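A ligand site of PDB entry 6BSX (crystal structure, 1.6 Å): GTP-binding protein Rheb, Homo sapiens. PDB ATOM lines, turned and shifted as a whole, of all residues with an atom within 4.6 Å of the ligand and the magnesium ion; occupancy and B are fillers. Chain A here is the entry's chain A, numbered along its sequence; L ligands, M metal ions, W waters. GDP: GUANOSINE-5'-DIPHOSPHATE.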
ATOM      1  N   TYR A  15      -7.750  -1.266   6.842  1.00  0.00           N
ATOM      2  CA  TYR A  15      -7.231  -0.655   5.624  1.00  0.00           C
ATOM      3  C   TYR A  15      -5.708  -0.500   5.658  1.00  0.00           C
ATOM      4  O   TYR A  15      -5.070  -0.465   6.726  1.00  0.00           O
ATOM      5  CB  TYR A  15      -7.904   0.701   5.485  1.00  0.00           C
ATOM      6  CG  TYR A  15      -7.698   1.445   4.183  1.00  0.00           C
ATOM      7  CD1 TYR A  15      -8.100   0.895   2.969  1.00  0.00           C
ATOM      8  CD2 TYR A  15      -7.116   2.699   4.186  1.00  0.00           C
ATOM      9  CE1 TYR A  15      -7.930   1.620   1.775  1.00  0.00           C
ATOM     10  CE2 TYR A  15      -6.958   3.425   3.020  1.00  0.00           C
ATOM     11  CZ  TYR A  15      -7.343   2.885   1.820  1.00  0.00           C
ATOM     12  OH  TYR A  15      -7.141   3.685   0.688  1.00  0.00           O
ATOM     13  N   ARG A  16      -5.124  -0.393   4.458  1.00  0.00           N
ATOM     14  CA  ARG A  16      -3.698  -0.119   4.327  1.00  0.00           C
ATOM     15  C   ARG A  16      -3.254   1.066   5.150  1.00  0.00           C
ATOM     16  O   ARG A  16      -3.933   2.119   5.198  1.00  0.00           O
ATOM     17  CB  ARG A  16      -3.328   0.123   2.871  1.00  0.00           C
ATOM     18  N   SER A  17      -2.121   0.888   5.812  1.00  0.00           N
ATOM     19  CA  SER A  17      -1.353   1.968   6.442  1.00  0.00           C
ATOM     20  C   SER A  17      -1.906   2.441   7.778  1.00  0.00           C
ATOM     21  O   SER A  17      -1.410   3.443   8.326  1.00  0.00           O
ATOM     22  CB  SER A  17      -1.193   3.146   5.473  1.00  0.00           C
ATOM     23  OG  SER A  17      -0.432   2.720   4.363  1.00  0.00           O
ATOM     24  N   VAL A  18      -2.899   1.745   8.324  1.00  0.00           N
ATOM     25  CA  VAL A  18      -3.478   2.227   9.612  1.00  0.00           C
ATOM     26  C   VAL A  18      -2.596   1.918  10.808  1.00  0.00           C
ATOM     27  O   VAL A  18      -2.777   2.447  11.906  1.00  0.00           O
ATOM     28  CB  VAL A  18      -4.907   1.623   9.841  1.00  0.00           C
ATOM     29  CG1 VAL A  18      -5.859   2.059   8.683  1.00  0.00           C
ATOM     30  CG2 VAL A  18      -4.846   0.066  10.050  1.00  0.00           C
ATOM     31  N   GLY A  19      -1.666   0.991  10.623  1.00  0.00           N
ATOM     32  CA  GLY A  19      -0.663   0.684  11.641  1.00  0.00           C
ATOM     33  C   GLY A  19      -0.828  -0.719  12.179  1.00  0.00           C
ATOM     34  O   GLY A  19      -0.380  -0.990  13.290  1.00  0.00           O
ATOM     35  N   LYS A  20      -1.468  -1.595  11.411  1.00  0.00           N
ATOM     36  CA  LYS A  20      -1.647  -2.991  11.896  1.00  0.00           C
ATOM     37  C   LYS A  20      -0.268  -3.656  12.222  1.00  0.00           C
ATOM     38  O   LYS A  20      -0.071  -4.220  13.354  1.00  0.00           O
ATOM     39  CB  LYS A  20      -2.436  -3.828  10.879  1.00  0.00           C
ATOM     40  CG  LYS A  20      -3.887  -3.413  10.575  1.00  0.00           C
ATOM     41  CD  LYS A  20      -4.462  -4.383   9.511  1.00  0.00           C
ATOM     42  CE  LYS A  20      -3.564  -4.431   8.284  1.00  0.00           C
ATOM     43  NZ  LYS A  20      -3.559  -3.157   7.430  1.00  0.00           N
ATOM     44  N   SER A  21       0.713  -3.625  11.275  1.00  0.00           N
ATOM     45  CA  SER A  21       2.040  -4.176  11.577  1.00  0.00           C
ATOM     46  C   SER A  21       2.725  -3.498  12.706  1.00  0.00           C
ATOM     47  O   SER A  21       3.295  -4.155  13.554  1.00  0.00           O
ATOM     48  CB  SER A  21       2.939  -4.132  10.334  1.00  0.00           C
ATOM     49  OG  SER A  21       2.288  -4.863   9.368  1.00  0.00           O
ATOM     50  N   SER A  22       2.616  -2.177  12.763  1.00  0.00           N
ATOM     51  CA  SER A  22       3.362  -1.439  13.780  1.00  0.00           C
ATOM     52  C   SER A  22       2.812  -1.695  15.180  1.00  0.00           C
ATOM     53  O   SER A  22       3.576  -1.790  16.143  1.00  0.00           O
ATOM     54  CB  SER A  22       3.326   0.040  13.478  1.00  0.00           C
ATOM     55  OG  SER A  22       4.003   0.330  12.269  1.00  0.00           O
ATOM     56  N   PHE A  32       8.984   0.163  17.934  1.00  0.00           N
ATOM     57  CA  PHE A  32       8.241   0.818  16.843  1.00  0.00           C
ATOM     58  C   PHE A  32       9.100   0.707  15.587  1.00  0.00           C
ATOM     59  O   PHE A  32      10.156   1.334  15.489  1.00  0.00           O
ATOM     60  CB  PHE A  32       7.922   2.284  17.183  1.00  0.00           C
ATOM     61  CG  PHE A  32       7.205   3.049  16.068  1.00  0.00           C
ATOM     62  CD1 PHE A  32       5.904   2.746  15.746  1.00  0.00           C
ATOM     63  CD2 PHE A  32       7.849   4.054  15.376  1.00  0.00           C
ATOM     64  CE1 PHE A  32       5.213   3.454  14.722  1.00  0.00           C
ATOM     65  CE2 PHE A  32       7.172   4.778  14.358  1.00  0.00           C
ATOM     66  CZ  PHE A  32       5.867   4.461  14.016  1.00  0.00           C
ATOM     67  N   VAL A  33       8.688  -0.111  14.633  1.00  0.00           N
ATOM     68  CA  VAL A  33       9.574  -0.379  13.513  1.00  0.00           C
ATOM     69  C   VAL A  33       9.550   0.794  12.545  1.00  0.00           C
ATOM     70  O   VAL A  33       8.494   1.376  12.296  1.00  0.00           O
ATOM     71  CB  VAL A  33       9.233  -1.671  12.753  1.00  0.00           C
ATOM     72  CG1 VAL A  33       9.722  -2.895  13.523  1.00  0.00           C
ATOM     73  CG2 VAL A  33       7.737  -1.761  12.437  1.00  0.00           C
ATOM     74  N   ASP A  34      10.725   1.115  12.004  1.00  0.00           N
ATOM     75  CA  ASP A  34      10.857   2.163  10.998  1.00  0.00           C
ATOM     76  C   ASP A  34       9.868   1.910   9.880  1.00  0.00           C
ATOM     77  O   ASP A  34       8.985   2.740   9.604  1.00  0.00           O
ATOM     78  CB  ASP A  34      12.291   2.206  10.453  1.00  0.00           C
ATOM     79  N   TYR A  36       7.817  -1.664   7.759  1.00  0.00           N
ATOM     80  CA  TYR A  36       7.599  -3.088   7.620  1.00  0.00           C
ATOM     81  C   TYR A  36       6.761  -3.309   6.358  1.00  0.00           C
ATOM     82  O   TYR A  36       5.782  -2.607   6.139  1.00  0.00           O
ATOM     83  CB  TYR A  36       6.920  -3.638   8.872  1.00  0.00           C
ATOM     84  CG  TYR A  36       6.569  -5.109   8.838  1.00  0.00           C
ATOM     85  CD1 TYR A  36       7.435  -6.072   9.351  1.00  0.00           C
ATOM     86  CD2 TYR A  36       5.341  -5.519   8.332  1.00  0.00           C
ATOM     87  CE1 TYR A  36       7.082  -7.419   9.347  1.00  0.00           C
ATOM     88  CE2 TYR A  36       4.974  -6.809   8.331  1.00  0.00           C
ATOM     89  CZ  TYR A  36       5.862  -7.774   8.825  1.00  0.00           C
ATOM     90  OH  TYR A  36       5.474  -9.067   8.816  1.00  0.00           O
ATOM     91  N   ASP A  37       7.224  -4.242   5.524  1.00  0.00           N
ATOM     92  CA  ASP A  37       6.602  -4.525   4.212  1.00  0.00           C
ATOM     93  C   ASP A  37       5.074  -4.525   4.252  1.00  0.00           C
ATOM     94  O   ASP A  37       4.474  -5.384   4.865  1.00  0.00           O
ATOM     95  CB  ASP A  37       7.122  -5.899   3.679  1.00  0.00           C
ATOM     96  CG  ASP A  37       6.813  -6.144   2.170  1.00  0.00           C
ATOM     97  OD1 ASP A  37       5.874  -5.525   1.608  1.00  0.00           O
ATOM     98  OD2 ASP A  37       7.535  -6.970   1.511  1.00  0.00           O
ATOM     99  N   PRO A  38       4.418  -3.586   3.544  1.00  0.00           N
ATOM    100  CA  PRO A  38       2.949  -3.499   3.647  1.00  0.00           C
ATOM    101  C   PRO A  38       2.201  -4.623   2.983  1.00  0.00           C
ATOM    102  O   PRO A  38       0.992  -4.770   3.182  1.00  0.00           O
ATOM    103  CB  PRO A  38       2.596  -2.165   2.955  1.00  0.00           C
ATOM    104  CG  PRO A  38       3.818  -1.726   2.270  1.00  0.00           C
ATOM    105  CD  PRO A  38       5.008  -2.462   2.821  1.00  0.00           C
ATOM    106  N   ASP A  61      -1.208 -10.643  11.497  1.00  0.00           N
ATOM    107  CA  ASP A  61      -1.035  -9.282  10.966  1.00  0.00           C
ATOM    108  C   ASP A  61      -1.323  -9.307   9.479  1.00  0.00           C
ATOM    109  O   ASP A  61      -0.410  -9.491   8.671  1.00  0.00           O
ATOM    110  CB  ASP A  61       0.392  -8.799  11.268  1.00  0.00           C
ATOM    111  CG  ASP A  61       0.712  -7.446  10.643  1.00  0.00           C
ATOM    112  OD1 ASP A  61      -0.229  -6.587  10.522  1.00  0.00           O
ATOM    113  OD2 ASP A  61       1.919  -7.195  10.304  1.00  0.00           O
ATOM    114  N   THR A  62      -2.593  -9.122   9.114  1.00  0.00           N
ATOM    115  CA  THR A  62      -3.010  -9.204   7.713  1.00  0.00           C
ATOM    116  C   THR A  62      -2.495  -8.034   6.882  1.00  0.00           C
ATOM    117  O   THR A  62      -2.184  -6.963   7.440  1.00  0.00           O
ATOM    118  CB  THR A  62      -4.542  -9.264   7.547  1.00  0.00           C
ATOM    119  OG1 THR A  62      -5.110  -7.976   7.881  1.00  0.00           O
ATOM    120  CG2 THR A  62      -5.156 -10.362   8.415  1.00  0.00           C
ATOM    121  N   ASN A 120      -6.169   3.765  15.802  1.00  0.00           N
ATOM    122  CA  ASN A 120      -4.731   3.912  15.989  1.00  0.00           C
ATOM    123  C   ASN A 120      -4.153   5.250  15.524  1.00  0.00           C
ATOM    124  O   ASN A 120      -4.883   6.062  14.940  1.00  0.00           O
ATOM    125  CB  ASN A 120      -4.028   2.716  15.262  1.00  0.00           C
ATOM    126  CG  ASN A 120      -2.561   2.677  15.554  1.00  0.00           C
ATOM    127  OD1 ASN A 120      -2.148   2.626  16.740  1.00  0.00           O
ATOM    128  ND2 ASN A 120      -1.750   2.551  14.483  1.00  0.00           N
ATOM    129  N   LYS A 121      -2.875   5.506  15.859  1.00  0.00           N
ATOM    130  CA  LYS A 121      -2.133   6.726  15.578  1.00  0.00           C
ATOM    131  C   LYS A 121      -2.644   7.908  16.424  1.00  0.00           C
ATOM    132  O   LYS A 121      -2.573   9.033  15.968  1.00  0.00           O
ATOM    133  CB  LYS A 121      -2.211   7.130  14.094  1.00  0.00           C
ATOM    134  CG  LYS A 121      -1.645   5.998  13.180  1.00  0.00           C
ATOM    135  CD  LYS A 121      -1.367   6.487  11.746  1.00  0.00           C
ATOM    136  CE  LYS A 121      -1.111   5.312  10.806  1.00  0.00           C
ATOM    137  NZ  LYS A 121      -0.599   5.867   9.518  1.00  0.00           N
ATOM    138  N   ASP A 123      -1.290   9.443  18.630  1.00  0.00           N
ATOM    139  CA  ASP A 123      -0.181  10.357  18.927  1.00  0.00           C
ATOM    140  C   ASP A 123      -0.109  11.511  17.919  1.00  0.00           C
ATOM    141  O   ASP A 123       0.533  12.510  18.207  1.00  0.00           O
ATOM    142  CB  ASP A 123       1.169   9.591  18.979  1.00  0.00           C
ATOM    143  CG  ASP A 123       1.516   8.918  17.660  1.00  0.00           C
ATOM    144  OD1 ASP A 123       0.823   7.935  17.337  1.00  0.00           O
ATOM    145  OD2 ASP A 123       2.433   9.374  16.961  1.00  0.00           O
ATOM    146  N   LEU A 124      -0.767  11.377  16.759  1.00  0.00           N
ATOM    147  CA  LEU A 124      -0.680  12.379  15.713  1.00  0.00           C
ATOM    148  C   LEU A 124      -1.783  13.443  15.912  1.00  0.00           C
ATOM    149  O   LEU A 124      -2.731  13.507  15.126  1.00  0.00           O
ATOM    150  CB  LEU A 124      -0.782  11.727  14.339  1.00  0.00           C
ATOM    151  CG  LEU A 124       0.406  10.814  13.993  1.00  0.00           C
ATOM    152  CD1 LEU A 124       0.221  10.176  12.603  1.00  0.00           C
ATOM    153  CD2 LEU A 124       1.738  11.555  14.071  1.00  0.00           C
ATOM    154  N   SER A 149      -5.137   3.691  20.280  1.00  0.00           N
ATOM    155  CA  SER A 149      -3.753   3.307  20.501  1.00  0.00           C
ATOM    156  C   SER A 149      -2.799   4.186  19.741  1.00  0.00           C
ATOM    157  O   SER A 149      -3.185   4.898  18.827  1.00  0.00           O
ATOM    158  CB  SER A 149      -3.536   1.873  20.040  1.00  0.00           C
ATOM    159  OG  SER A 149      -3.910   1.816  18.666  1.00  0.00           O
ATOM    160  N   SER A 150      -1.523   4.084  20.107  1.00  0.00           N
ATOM    161  CA  SER A 150      -0.394   4.559  19.300  1.00  0.00           C
ATOM    162  C   SER A 150       0.607   3.425  19.219  1.00  0.00           C
ATOM    163  O   SER A 150       1.044   2.963  20.275  1.00  0.00           O
ATOM    164  CB  SER A 150       0.270   5.770  19.920  1.00  0.00           C
ATOM    165  OG  SER A 150       1.456   6.117  19.247  1.00  0.00           O
ATOM    166  N   ALA A 151       1.016   3.001  18.015  1.00  0.00           N
ATOM    167  CA  ALA A 151       2.066   2.003  17.908  1.00  0.00           C
ATOM    168  C   ALA A 151       3.428   2.504  18.447  1.00  0.00           C
ATOM    169  O   ALA A 151       4.363   1.706  18.607  1.00  0.00           O
ATOM    170  CB  ALA A 151       2.191   1.528  16.473  1.00  0.00           C
ATOM    171  N   LYS A 152       3.523   3.811  18.753  1.00  0.00           N
ATOM    172  CA  LYS A 152       4.738   4.345  19.389  1.00  0.00           C
ATOM    173  C   LYS A 152       4.699   4.196  20.907  1.00  0.00           C
ATOM    174  O   LYS A 152       5.687   4.504  21.562  1.00  0.00           O
ATOM    175  CB  LYS A 152       4.966   5.823  19.037  1.00  0.00           C
ATOM    176  CG  LYS A 152       5.308   6.079  17.562  1.00  0.00           C
ATOM    177  CD  LYS A 152       5.538   7.576  17.294  1.00  0.00           C
ATOM    178  CE  LYS A 152       6.112   7.781  15.904  1.00  0.00           C
ATOM    179  NZ  LYS A 152       6.809   9.096  15.755  1.00  0.00           N
HETATM  180  PB  GDP L   1      -0.302  -1.484   8.013  1.00  0.00           P
HETATM  181  O1B GDP L   1      -1.628  -1.405   8.604  1.00  0.00           O
HETATM  182  O2B GDP L   1       0.543  -2.691   8.501  1.00  0.00           O
HETATM  183  O3B GDP L   1      -0.288  -1.307   6.532  1.00  0.00           O
HETATM  184  O3A GDP L   1       0.492  -0.173   8.671  1.00  0.00           O
HETATM  185  PA  GDP L   1       1.954  -0.033   9.113  1.00  0.00           P
HETATM  186  O1A GDP L   1       2.252  -0.606  10.478  1.00  0.00           O
HETATM  187  O2A GDP L   1       2.997  -0.283   8.046  1.00  0.00           O
HETATM  188  O5' GDP L   1       2.089   1.690   9.317  1.00  0.00           O
HETATM  189  C5' GDP L   1       1.876   2.484   8.224  1.00  0.00           C
HETATM  190  C4' GDP L   1       2.704   3.773   8.435  1.00  0.00           C
HETATM  191  O4' GDP L   1       2.140   4.441   9.665  1.00  0.00           O
HETATM  192  C3' GDP L   1       4.176   3.509   8.693  1.00  0.00           C
HETATM  193  O3' GDP L   1       4.886   4.631   8.117  1.00  0.00           O
HETATM  194  C2' GDP L   1       4.248   3.526  10.236  1.00  0.00           C
HETATM  195  O2' GDP L   1       5.480   3.950  10.726  1.00  0.00           O
HETATM  196  C1' GDP L   1       3.143   4.568  10.603  1.00  0.00           C
HETATM  197  N9  GDP L   1       2.437   4.270  11.876  1.00  0.00           N
HETATM  198  C8  GDP L   1       1.732   3.138  12.274  1.00  0.00           C
HETATM  199  N7  GDP L   1       1.177   3.254  13.497  1.00  0.00           N
HETATM  200  C5  GDP L   1       1.502   4.537  13.905  1.00  0.00           C
HETATM  201  C6  GDP L   1       1.152   5.168  15.138  1.00  0.00           C
HETATM  202  O6  GDP L   1       0.463   4.788  16.087  1.00  0.00           O
HETATM  203  N1  GDP L   1       1.665   6.503  15.150  1.00  0.00           N
HETATM  204  C2  GDP L   1       2.414   7.063  14.139  1.00  0.00           C
HETATM  205  N2  GDP L   1       2.835   8.378  14.334  1.00  0.00           N
HETATM  206  N3  GDP L   1       2.731   6.502  12.971  1.00  0.00           N
HETATM  207  C4  GDP L   1       2.244   5.210  12.918  1.00  0.00           C
HETATM  208 MG    MG M   1       1.404  -4.253   7.524  1.00  0.00          MG
HETATM  209  O   HOH W   1       2.282  -5.756   6.532  1.00  0.00           O
HETATM  210  O   HOH W   2       5.303   0.350   7.783  1.00  0.00           O
HETATM  211  O   HOH W   3       4.347   0.376   5.521  1.00  0.00           O
HETATM  212  O   HOH W   4       1.436   0.205   5.297  1.00  0.00           O
HETATM  213  O   HOH W   5       0.265  -3.785   5.820  1.00  0.00           O
HETATM  214  O   HOH W   6       4.996   9.635  12.890  1.00  0.00           O
HETATM  215  O   HOH W   7      -0.146  -5.537   8.174  1.00  0.00           O
HETATM  216  O   HOH W   8       2.952  -3.041   7.145  1.00  0.00           O
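O3A of the ligand sits at hydrogen-bond distance from N of Gly 19. An oxygen (O1B) of the ligand sits at hydrogen-bond distance from the backbone NH (N) of Lys 20, 2.8 Å away. O4' of the ligand sits at hydrogen-bond distance from NZ of Lys 121, 3.1 Å away. OD1 of Asp 123 sits at hydrogen-bond distance from N1 of the ligand (2.7 Å). An oxygen (O6) of the ligand sits at hydrogen-bond distance from the backbone NH of Ala 151 (2.7 Å). The side-chain hydroxyl (OG) of Ser 22 sits at hydrogen-bond distance from an oxygen (O1A) of the ligand (2.7 Å). O3B of the ligand is in hydrogen-bond range of N of Ser 17 (2.9 Å). The backbone NH (N) of Val 18 is in hydrogen-bond range of an oxygen (O1B) of the ligand (3.4 Å). The side-chain amino group (NZ) of Lys 20 is in salt-bridge range of an oxygen (O1B) of the ligand, 2.9 Å away. ND2 of Asn 120 lies within hydrogen-bond range of N7 of the ligand (3.2 Å). The backbone NH (N) of Ser 21 lies within hydrogen-bond range of an oxygen (O1A) of the ligand. O1A of the ligand is in hydrogen-bond range of N of Ser 22, at 2.8 Å. O6 of the ligand lies close to N of Lys 121 (3.4 Å).
The side-chain carboxylate (OD1) of Asp 61 sits at hydrogen-bond distance from the backbone NH (N) of Ser 21. OD1 of Asn 120 is in hydrogen-bond range of N of Ala 151 (3.4 Å). The side-chain hydroxyl (OG) of Ser 150 sits close to the backbone NH (N) of Lys 152 (3.1 Å). The backbone carbonyl oxygen (O) of Ser 17 sits at hydrogen-bond distance from the side-chain amino group (NZ) of Lys 121 (2.8 Å). The side-chain amide nitrogen (ND2) of Asn 120 is in hydrogen-bond range of the backbone carbonyl oxygen (O) of Val 18 (2.8 Å). The backbone NH (N) of Lys 121 is in hydrogen-bond range of the backbone carbonyl oxygen (O) of Ser 149 (3.0 Å). O of Tyr 15 sits at hydrogen-bond distance from NZ of Lys 20, 3.2 Å away. The side-chain amide oxygen (OD1) of Asn 120 is in hydrogen-bond range of the side-chain hydroxyl (OG) of Ser 149, at 2.7 Å.
Residues that only touch the ligand: Ser 150 (3.3 Å), Phe 32 (3.4 Å), Leu 124 (3.4 Å), Lys 152 (3.7 Å) and Asp 34 (3.9 Å). Within 4 Å of the ligand: Ser 17, Val 18, Gly 19, Lys 20, Ser 21, Ser 22, Phe 32, Asp 34, Asn 120, Lys 121, Asp 123, Leu 124, Ser 150, Ala 151 and Lys 152.
The nearest printed residue that does not touch the magnesium ion is Asp 61 (4.1 Å).
The magnesium ion is bound by water W8 (2.0 Å), water W1 (2.0 Å), O2B of the ligand (2.0 Å), water W5 (2.1 Å), water W7 (2.1 Å) and OG of Ser 21 (2.1 Å).
Water W7 lies within hydrogen-bond range of OD1 of Asp 61 (2.6 Å) and O of Thr 62 (2.6 Å). Water W8 bridges an oxygen (O2A) of the ligand and the backbone carbonyl oxygen of Tyr 36. Water W2 bridges an oxygen (O2A) of the ligand and the backbone NH of Tyr 36. Water W4 lies within hydrogen-bond range of an oxygen (O3B) of the ligand (2.6 Å) and the side-chain hydroxyl (OG) of Ser 17 (3.3 Å). Water W6 lies within hydrogen-bond range of N2 of the ligand (2.9 Å) and NZ of Lys 152 (3.4 Å). Water W3 lies within hydrogen-bond range of O2A of the ligand and O of Tyr 36.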
